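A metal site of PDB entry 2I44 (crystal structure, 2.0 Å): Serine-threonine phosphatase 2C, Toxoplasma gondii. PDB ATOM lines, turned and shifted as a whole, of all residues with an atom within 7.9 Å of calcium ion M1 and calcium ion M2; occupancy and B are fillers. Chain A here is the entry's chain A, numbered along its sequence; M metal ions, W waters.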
ATOM      1  N   ARG A  33     -18.425  12.325  33.763  1.00  0.00           N
ATOM      2  CA  ARG A  33     -18.166  11.192  34.647  1.00  0.00           C
ATOM      3  C   ARG A  33     -17.451  11.665  35.922  1.00  0.00           C
ATOM      4  O   ARG A  33     -16.832  12.729  35.936  1.00  0.00           O
ATOM      5  CB  ARG A  33     -17.325  10.137  33.932  1.00  0.00           C
ATOM      6  CG  ARG A  33     -17.767   9.860  32.495  1.00  0.00           C
ATOM      7  CD  ARG A  33     -19.178   9.304  32.379  1.00  0.00           C
ATOM      8  NE  ARG A  33     -19.228   7.844  32.400  1.00  0.00           N
ATOM      9  CZ  ARG A  33     -19.195   7.111  33.502  1.00  0.00           C
ATOM     10  NH1 ARG A  33     -19.118   7.696  34.689  1.00  0.00           N
ATOM     11  NH2 ARG A  33     -19.236   5.784  33.423  1.00  0.00           N
ATOM     12  N   HIS A  35     -14.955  10.134  37.228  1.00  0.00           N
ATOM     13  CA  HIS A  35     -13.544   9.777  37.072  1.00  0.00           C
ATOM     14  C   HIS A  35     -13.097   9.887  35.626  1.00  0.00           C
ATOM     15  O   HIS A  35     -13.913   9.765  34.706  1.00  0.00           O
ATOM     16  CB  HIS A  35     -13.320   8.326  37.504  1.00  0.00           C
ATOM     17  CG  HIS A  35     -13.491   8.078  38.970  1.00  0.00           C
ATOM     18  ND1 HIS A  35     -13.634   6.801  39.481  1.00  0.00           N
ATOM     19  CD2 HIS A  35     -13.506   8.918  40.025  1.00  0.00           C
ATOM     20  CE1 HIS A  35     -13.718   6.868  40.789  1.00  0.00           C
ATOM     21  NE2 HIS A  35     -13.636   8.141  41.152  1.00  0.00           N
ATOM     22  N   GLN A  36     -11.807  10.082  35.417  1.00  0.00           N
ATOM     23  CA  GLN A  36     -11.242  10.127  34.065  1.00  0.00           C
ATOM     24  C   GLN A  36     -10.544   8.783  33.925  1.00  0.00           C
ATOM     25  O   GLN A  36      -9.449   8.585  34.478  1.00  0.00           O
ATOM     26  CB  GLN A  36     -10.245  11.265  33.926  1.00  0.00           C
ATOM     27  CG  GLN A  36      -9.454  11.279  32.613  1.00  0.00           C
ATOM     28  CD  GLN A  36     -10.340  11.143  31.372  1.00  0.00           C
ATOM     29  OE1 GLN A  36     -10.877  10.063  31.102  1.00  0.00           O
ATOM     30  NE2 GLN A  36     -10.490  12.236  30.626  1.00  0.00           N
ATOM     31  N   GLU A  37     -11.173   7.852  33.217  1.00  0.00           N
ATOM     32  CA  GLU A  37     -10.601   6.523  33.064  1.00  0.00           C
ATOM     33  C   GLU A  37     -10.047   6.218  31.681  1.00  0.00           C
ATOM     34  O   GLU A  37      -9.682   5.083  31.390  1.00  0.00           O
ATOM     35  CB  GLU A  37     -11.643   5.485  33.480  1.00  0.00           C
ATOM     36  CG  GLU A  37     -12.320   5.855  34.791  1.00  0.00           C
ATOM     37  CD  GLU A  37     -13.070   4.711  35.445  1.00  0.00           C
ATOM     38  OE1 GLU A  37     -13.757   3.945  34.737  1.00  0.00           O
ATOM     39  OE2 GLU A  37     -12.982   4.585  36.696  1.00  0.00           O
ATOM     40  N   ASP A  38      -9.988   7.235  30.833  1.00  0.00           N
ATOM     41  CA  ASP A  38      -9.423   7.092  29.492  1.00  0.00           C
ATOM     42  C   ASP A  38      -7.923   7.347  29.630  1.00  0.00           C
ATOM     43  O   ASP A  38      -7.499   8.198  30.422  1.00  0.00           O
ATOM     44  CB  ASP A  38      -9.991   8.151  28.537  1.00  0.00           C
ATOM     45  CG  ASP A  38     -11.250   7.692  27.827  1.00  0.00           C
ATOM     46  OD1 ASP A  38     -11.828   6.636  28.174  1.00  0.00           O
ATOM     47  OD2 ASP A  38     -11.687   8.429  26.898  1.00  0.00           O
ATOM     48  N   PHE A  59      -6.781   3.989  25.399  1.00  0.00           N
ATOM     49  CA  PHE A  59      -7.373   2.972  26.260  1.00  0.00           C
ATOM     50  C   PHE A  59      -8.557   3.450  27.085  1.00  0.00           C
ATOM     51  O   PHE A  59      -8.445   4.388  27.870  1.00  0.00           O
ATOM     52  CB  PHE A  59      -6.285   2.436  27.208  1.00  0.00           C
ATOM     53  CG  PHE A  59      -4.981   2.159  26.512  1.00  0.00           C
ATOM     54  CD1 PHE A  59      -4.786   0.975  25.814  1.00  0.00           C
ATOM     55  CD2 PHE A  59      -3.957   3.101  26.532  1.00  0.00           C
ATOM     56  CE1 PHE A  59      -3.600   0.735  25.134  1.00  0.00           C
ATOM     57  CE2 PHE A  59      -2.755   2.876  25.850  1.00  0.00           C
ATOM     58  CZ  PHE A  59      -2.587   1.681  25.146  1.00  0.00           C
ATOM     59  N   ASP A  60      -9.701   2.788  26.910  1.00  0.00           N
ATOM     60  CA  ASP A  60     -10.907   3.144  27.667  1.00  0.00           C
ATOM     61  C   ASP A  60     -11.043   2.228  28.886  1.00  0.00           C
ATOM     62  O   ASP A  60     -11.461   1.076  28.774  1.00  0.00           O
ATOM     63  CB  ASP A  60     -12.168   3.011  26.779  1.00  0.00           C
ATOM     64  CG  ASP A  60     -13.433   3.544  27.459  1.00  0.00           C
ATOM     65  OD1 ASP A  60     -13.390   3.857  28.673  1.00  0.00           O
ATOM     66  OD2 ASP A  60     -14.479   3.638  26.775  1.00  0.00           O
ATOM     67  N   GLY A  61     -10.663   2.739  30.047  1.00  0.00           N
ATOM     68  CA  GLY A  61     -10.761   1.949  31.254  1.00  0.00           C
ATOM     69  C   GLY A  61     -12.155   1.946  31.838  1.00  0.00           C
ATOM     70  O   GLY A  61     -12.974   2.811  31.521  1.00  0.00           O
ATOM     71  N   THR A  62     -12.433   0.956  32.674  1.00  0.00           N
ATOM     72  CA  THR A  62     -13.728   0.836  33.335  1.00  0.00           C
ATOM     73  C   THR A  62     -13.512   0.107  34.668  1.00  0.00           C
ATOM     74  O   THR A  62     -12.639  -0.760  34.782  1.00  0.00           O
ATOM     75  CB  THR A  62     -14.745   0.067  32.464  1.00  0.00           C
ATOM     76  OG1 THR A  62     -15.980  -0.062  33.178  1.00  0.00           O
ATOM     77  CG2 THR A  62     -14.237  -1.313  32.142  1.00  0.00           C
ATOM     78  N   VAL A  63     -14.335   0.456  35.664  1.00  0.00           N
ATOM     79  CA  VAL A  63     -14.243  -0.094  37.011  1.00  0.00           C
ATOM     80  C   VAL A  63     -12.908   0.391  37.573  1.00  0.00           C
ATOM     81  O   VAL A  63     -12.028  -0.394  37.911  1.00  0.00           O
ATOM     82  CB  VAL A  63     -14.266  -1.650  37.043  1.00  0.00           C
ATOM     83  CG1 VAL A  63     -14.390  -2.124  38.475  1.00  0.00           C
ATOM     84  CG2 VAL A  63     -15.440  -2.173  36.209  1.00  0.00           C
ATOM     85  N   GLY A  64     -12.767   1.714  37.660  1.00  0.00           N
ATOM     86  CA  GLY A  64     -11.535   2.300  38.139  1.00  0.00           C
ATOM     87  C   GLY A  64     -10.605   2.523  36.960  1.00  0.00           C
ATOM     88  O   GLY A  64     -10.852   2.001  35.873  1.00  0.00           O
ATOM     89  N   SER A  68      -6.348   0.827  32.616  1.00  0.00           N
ATOM     90  CA  SER A  68      -5.905   1.763  31.578  1.00  0.00           C
ATOM     91  C   SER A  68      -4.651   2.536  31.996  1.00  0.00           C
ATOM     92  O   SER A  68      -3.744   2.756  31.192  1.00  0.00           O
ATOM     93  CB  SER A  68      -7.035   2.734  31.207  1.00  0.00           C
ATOM     94  OG  SER A  68      -7.452   3.505  32.318  1.00  0.00           O
ATOM     95  N   SER A 137     -10.630  -3.173  34.192  1.00  0.00           N
ATOM     96  CA  SER A 137     -10.408  -3.555  32.803  1.00  0.00           C
ATOM     97  C   SER A 137     -10.207  -2.330  31.911  1.00  0.00           C
ATOM     98  O   SER A 137     -10.352  -1.185  32.349  1.00  0.00           O
ATOM     99  CB  SER A 137     -11.615  -4.334  32.276  1.00  0.00           C
ATOM    100  OG  SER A 137     -11.930  -5.454  33.078  1.00  0.00           O
ATOM    101  N   SER A 138      -9.886  -2.583  30.642  1.00  0.00           N
ATOM    102  CA  SER A 138      -9.694  -1.513  29.681  1.00  0.00           C
ATOM    103  C   SER A 138      -9.779  -2.029  28.240  1.00  0.00           C
ATOM    104  O   SER A 138      -9.359  -3.157  27.933  1.00  0.00           O
ATOM    105  CB  SER A 138      -8.332  -0.838  29.894  1.00  0.00           C
ATOM    106  OG  SER A 138      -8.103   0.211  28.960  1.00  0.00           O
ATOM    107  N   THR A 139     -10.348  -1.215  27.360  1.00  0.00           N
ATOM    108  CA  THR A 139     -10.414  -1.588  25.963  1.00  0.00           C
ATOM    109  C   THR A 139      -9.059  -1.127  25.431  1.00  0.00           C
ATOM    110  O   THR A 139      -8.252  -0.552  26.167  1.00  0.00           O
ATOM    111  CB  THR A 139     -11.425  -0.768  25.180  1.00  0.00           C
ATOM    112  OG1 THR A 139     -10.994   0.599  25.164  1.00  0.00           O
ATOM    113  CG2 THR A 139     -12.813  -0.857  25.797  1.00  0.00           C
ATOM    114  N   ASP A 157     -14.395  -2.069  22.623  1.00  0.00           N
ATOM    115  CA  ASP A 157     -15.231  -1.259  21.763  1.00  0.00           C
ATOM    116  C   ASP A 157     -14.735   0.147  21.468  1.00  0.00           C
ATOM    117  O   ASP A 157     -15.530   1.028  21.166  1.00  0.00           O
ATOM    118  CB  ASP A 157     -16.657  -1.195  22.311  1.00  0.00           C
ATOM    119  CG  ASP A 157     -16.705  -0.749  23.742  1.00  0.00           C
ATOM    120  OD1 ASP A 157     -15.705  -0.160  24.217  1.00  0.00           O
ATOM    121  OD2 ASP A 157     -17.744  -0.966  24.381  1.00  0.00           O
ATOM    122  N   SER A 158     -13.428   0.367  21.601  1.00  0.00           N
ATOM    123  CA  SER A 158     -12.857   1.660  21.227  1.00  0.00           C
ATOM    124  C   SER A 158     -12.604   1.416  19.733  1.00  0.00           C
ATOM    125  O   SER A 158     -12.499   0.256  19.309  1.00  0.00           O
ATOM    126  CB  SER A 158     -11.528   1.926  21.945  1.00  0.00           C
ATOM    127  OG  SER A 158     -11.755   2.259  23.298  1.00  0.00           O
ATOM    128  N   TYR A 229     -18.307  -5.456  26.670  1.00  0.00           N
ATOM    129  CA  TYR A 229     -17.440  -5.864  25.579  1.00  0.00           C
ATOM    130  C   TYR A 229     -16.788  -7.177  26.015  1.00  0.00           C
ATOM    131  O   TYR A 229     -16.550  -7.393  27.207  1.00  0.00           O
ATOM    132  CB  TYR A 229     -16.407  -4.780  25.220  1.00  0.00           C
ATOM    133  CG  TYR A 229     -15.680  -4.116  26.367  1.00  0.00           C
ATOM    134  CD1 TYR A 229     -14.461  -4.608  26.821  1.00  0.00           C
ATOM    135  CD2 TYR A 229     -16.191  -2.969  26.961  1.00  0.00           C
ATOM    136  CE1 TYR A 229     -13.766  -3.968  27.848  1.00  0.00           C
ATOM    137  CE2 TYR A 229     -15.510  -2.320  27.989  1.00  0.00           C
ATOM    138  CZ  TYR A 229     -14.294  -2.824  28.424  1.00  0.00           C
ATOM    139  OH  TYR A 229     -13.599  -2.192  29.419  1.00  0.00           O
ATOM    140  N   THR A 265     -11.996   6.640  21.944  1.00  0.00           N
ATOM    141  CA  THR A 265     -12.838   5.805  22.786  1.00  0.00           C
ATOM    142  C   THR A 265     -14.302   5.949  22.355  1.00  0.00           C
ATOM    143  O   THR A 265     -14.625   6.830  21.546  1.00  0.00           O
ATOM    144  CB  THR A 265     -12.709   6.194  24.274  1.00  0.00           C
ATOM    145  OG1 THR A 265     -13.040   7.580  24.428  1.00  0.00           O
ATOM    146  CG2 THR A 265     -11.288   5.970  24.751  1.00  0.00           C
ATOM    147  N   ASP A 266     -15.167   5.106  22.904  1.00  0.00           N
ATOM    148  CA  ASP A 266     -16.585   5.155  22.553  1.00  0.00           C
ATOM    149  C   ASP A 266     -17.190   6.460  23.015  1.00  0.00           C
ATOM    150  O   ASP A 266     -18.309   6.814  22.625  1.00  0.00           O
ATOM    151  CB  ASP A 266     -17.352   3.953  23.145  1.00  0.00           C
ATOM    152  CG  ASP A 266     -17.338   3.912  24.681  1.00  0.00           C
ATOM    153  OD1 ASP A 266     -16.759   4.812  25.323  1.00  0.00           O
ATOM    154  OD2 ASP A 266     -17.913   2.958  25.229  1.00  0.00           O
ATOM    155  N   GLY A 267     -16.449   7.196  23.845  1.00  0.00           N
ATOM    156  CA  GLY A 267     -16.919   8.494  24.309  1.00  0.00           C
ATOM    157  C   GLY A 267     -17.123   9.399  23.095  1.00  0.00           C
ATOM    158  O   GLY A 267     -17.894  10.365  23.131  1.00  0.00           O
ATOM    159  N   LEU A 268     -16.414   9.073  22.015  1.00  0.00           N
ATOM    160  CA  LEU A 268     -16.530   9.812  20.767  1.00  0.00           C
ATOM    161  C   LEU A 268     -17.455   9.093  19.778  1.00  0.00           C
ATOM    162  O   LEU A 268     -18.354   9.706  19.195  1.00  0.00           O
ATOM    163  CB  LEU A 268     -15.169   9.991  20.092  1.00  0.00           C
ATOM    164  CG  LEU A 268     -15.279  10.481  18.637  1.00  0.00           C
ATOM    165  CD1 LEU A 268     -15.817  11.918  18.618  1.00  0.00           C
ATOM    166  CD2 LEU A 268     -13.926  10.427  17.945  1.00  0.00           C
ATOM    167  N   ASP A 270     -19.857   6.775  20.238  1.00  0.00           N
ATOM    168  CA  ASP A 270     -21.269   6.585  20.549  1.00  0.00           C
ATOM    169  C   ASP A 270     -22.066   7.754  19.992  1.00  0.00           C
ATOM    170  O   ASP A 270     -23.275   7.658  19.779  1.00  0.00           O
ATOM    171  CB  ASP A 270     -21.486   6.448  22.059  1.00  0.00           C
ATOM    172  CG  ASP A 270     -21.016   5.096  22.594  1.00  0.00           C
ATOM    173  OD1 ASP A 270     -20.894   4.139  21.787  1.00  0.00           O
ATOM    174  OD2 ASP A 270     -20.796   4.983  23.822  1.00  0.00           O
ATOM    175  N   ASP A 311     -19.660  10.986  28.308  1.00  0.00           N
ATOM    176  CA  ASP A 311     -18.732   9.980  28.814  1.00  0.00           C
ATOM    177  C   ASP A 311     -17.317  10.551  28.720  1.00  0.00           C
ATOM    178  O   ASP A 311     -17.135  11.643  28.186  1.00  0.00           O
ATOM    179  CB  ASP A 311     -18.840   8.723  27.965  1.00  0.00           C
ATOM    180  CG  ASP A 311     -17.892   7.622  28.407  1.00  0.00           C
ATOM    181  OD1 ASP A 311     -17.506   7.606  29.597  1.00  0.00           O
ATOM    182  OD2 ASP A 311     -17.531   6.772  27.564  1.00  0.00           O
ATOM    183  N   ASN A 312     -16.308   9.857  29.259  1.00  0.00           N
ATOM    184  CA  ASN A 312     -14.950  10.360  29.102  1.00  0.00           C
ATOM    185  C   ASN A 312     -14.779  10.327  27.575  1.00  0.00           C
ATOM    186  O   ASN A 312     -15.308   9.422  26.920  1.00  0.00           O
ATOM    187  CB  ASN A 312     -13.889   9.412  29.696  1.00  0.00           C
ATOM    188  CG  ASN A 312     -13.913   9.364  31.219  1.00  0.00           C
ATOM    189  OD1 ASN A 312     -14.322  10.309  31.887  1.00  0.00           O
ATOM    190  ND2 ASN A 312     -13.428   8.257  31.768  1.00  0.00           N
ATOM    191  N   ILE A 313     -14.055  11.297  27.022  1.00  0.00           N
ATOM    192  CA  ILE A 313     -13.843  11.356  25.585  1.00  0.00           C
ATOM    193  C   ILE A 313     -12.374  11.606  25.304  1.00  0.00           C
ATOM    194  O   ILE A 313     -11.772  12.526  25.850  1.00  0.00           O
ATOM    195  CB  ILE A 313     -14.650  12.501  24.916  1.00  0.00           C
ATOM    196  CG1 ILE A 313     -16.102  12.463  25.373  1.00  0.00           C
ATOM    197  CG2 ILE A 313     -14.586  12.352  23.390  1.00  0.00           C
ATOM    198  CD1 ILE A 313     -16.935  13.634  24.872  1.00  0.00           C
ATOM    199  N   THR A 314     -11.794  10.766  24.453  1.00  0.00           N
ATOM    200  CA  THR A 314     -10.403  10.884  24.074  1.00  0.00           C
ATOM    201  C   THR A 314     -10.261  10.667  22.578  1.00  0.00           C
ATOM    202  O   THR A 314     -10.812   9.710  22.025  1.00  0.00           O
ATOM    203  CB  THR A 314      -9.528   9.856  24.820  1.00  0.00           C
ATOM    204  OG1 THR A 314      -9.524  10.166  26.222  1.00  0.00           O
ATOM    205  CG2 THR A 314      -8.097   9.865  24.309  1.00  0.00           C
HETATM  206 CA    CA M   1     -16.090   4.974  27.538  1.00  0.00          CA
HETATM  207 CA    CA M   2     -14.507   4.062  30.563  1.00  0.00          CA
HETATM  208  O   HOH W   1     -15.960   2.338  30.000  1.00  0.00           O
HETATM  209  O   HOH W   2     -15.010   4.683  32.695  1.00  0.00           O
HETATM  210  O   HOH W   3     -13.260   5.867  30.576  1.00  0.00           O
HETATM  211  O   HOH W   4     -14.554   6.639  27.039  1.00  0.00           O
HETATM  212  O   HOH W   5     -15.945   5.245  29.607  1.00  0.00           O
HETATM  213  O   HOH W   6     -17.067   3.299  27.608  1.00  0.00           O
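Along chain A the residues within 4 Å of calcium ion M2 span positions 60 to 61.
The backbone NH (N) of Gly 61 is in hydrogen-bond range of the backbone carbonyl oxygen (O) of Glu 37, at 2.9 Å.
The backbone carbonyl oxygen of Asp 60 lies within hydrogen-bond range of the backbone NH of Thr 139, 2.9 Å away.
The backbone carbonyl oxygen (O) of Asp 60 sits close to the side-chain hydroxyl (OG) of Ser 138 (3.5 Å).
The guanidinium group of Arg 33 lies within salt-bridge range of the side-chain carboxylate of Asp 311 (3.3 Å).
Water W6 binds calcium ion M1, at 1.9 Å.
Calcium ion M1 is bound by water W5 (2.1 Å).
OD2 of Asp 60 is bound to calcium ion M1, at 2.2 Å.
Calcium ion M1 is bound by the side-chain carboxylate (OD2) of Asp 311, at 2.3 Å.
The side-chain carboxylate (OD1) of Asp 266 is bound to calcium ion M1.
Water W4 binds calcium ion M1, 2.3 Å away.
Calcium ion M1 has six donor atoms within binding distance.
Slightly farther from calcium ion M1 lies the side-chain carboxylate (OD1) of Asp 60 (3.1 Å).
Water W5 binds calcium ion M2, 2.1 Å away.
Water W3 binds calcium ion M2.
O of Gly 61 is bound to calcium ion M2, 2.2 Å away.
OD1 of Asp 60 binds calcium ion M2 (2.2 Å).
Water W2 is bound to calcium ion M2 (2.3 Å).
Water W1 is bound to calcium ion M2.
Calcium ion M2 has six donor atoms within binding distance.
Water W4 lies within hydrogen-bond range of the backbone carbonyl oxygen of Asn 312 (2.9 Å), the side-chain carboxylate of Asp 38 (3.0 Å) and the side-chain hydroxyl of Thr 265 (3.2 Å).
Water W3 bridges ND2 of Asn 312 and OD1 of Asp 38.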
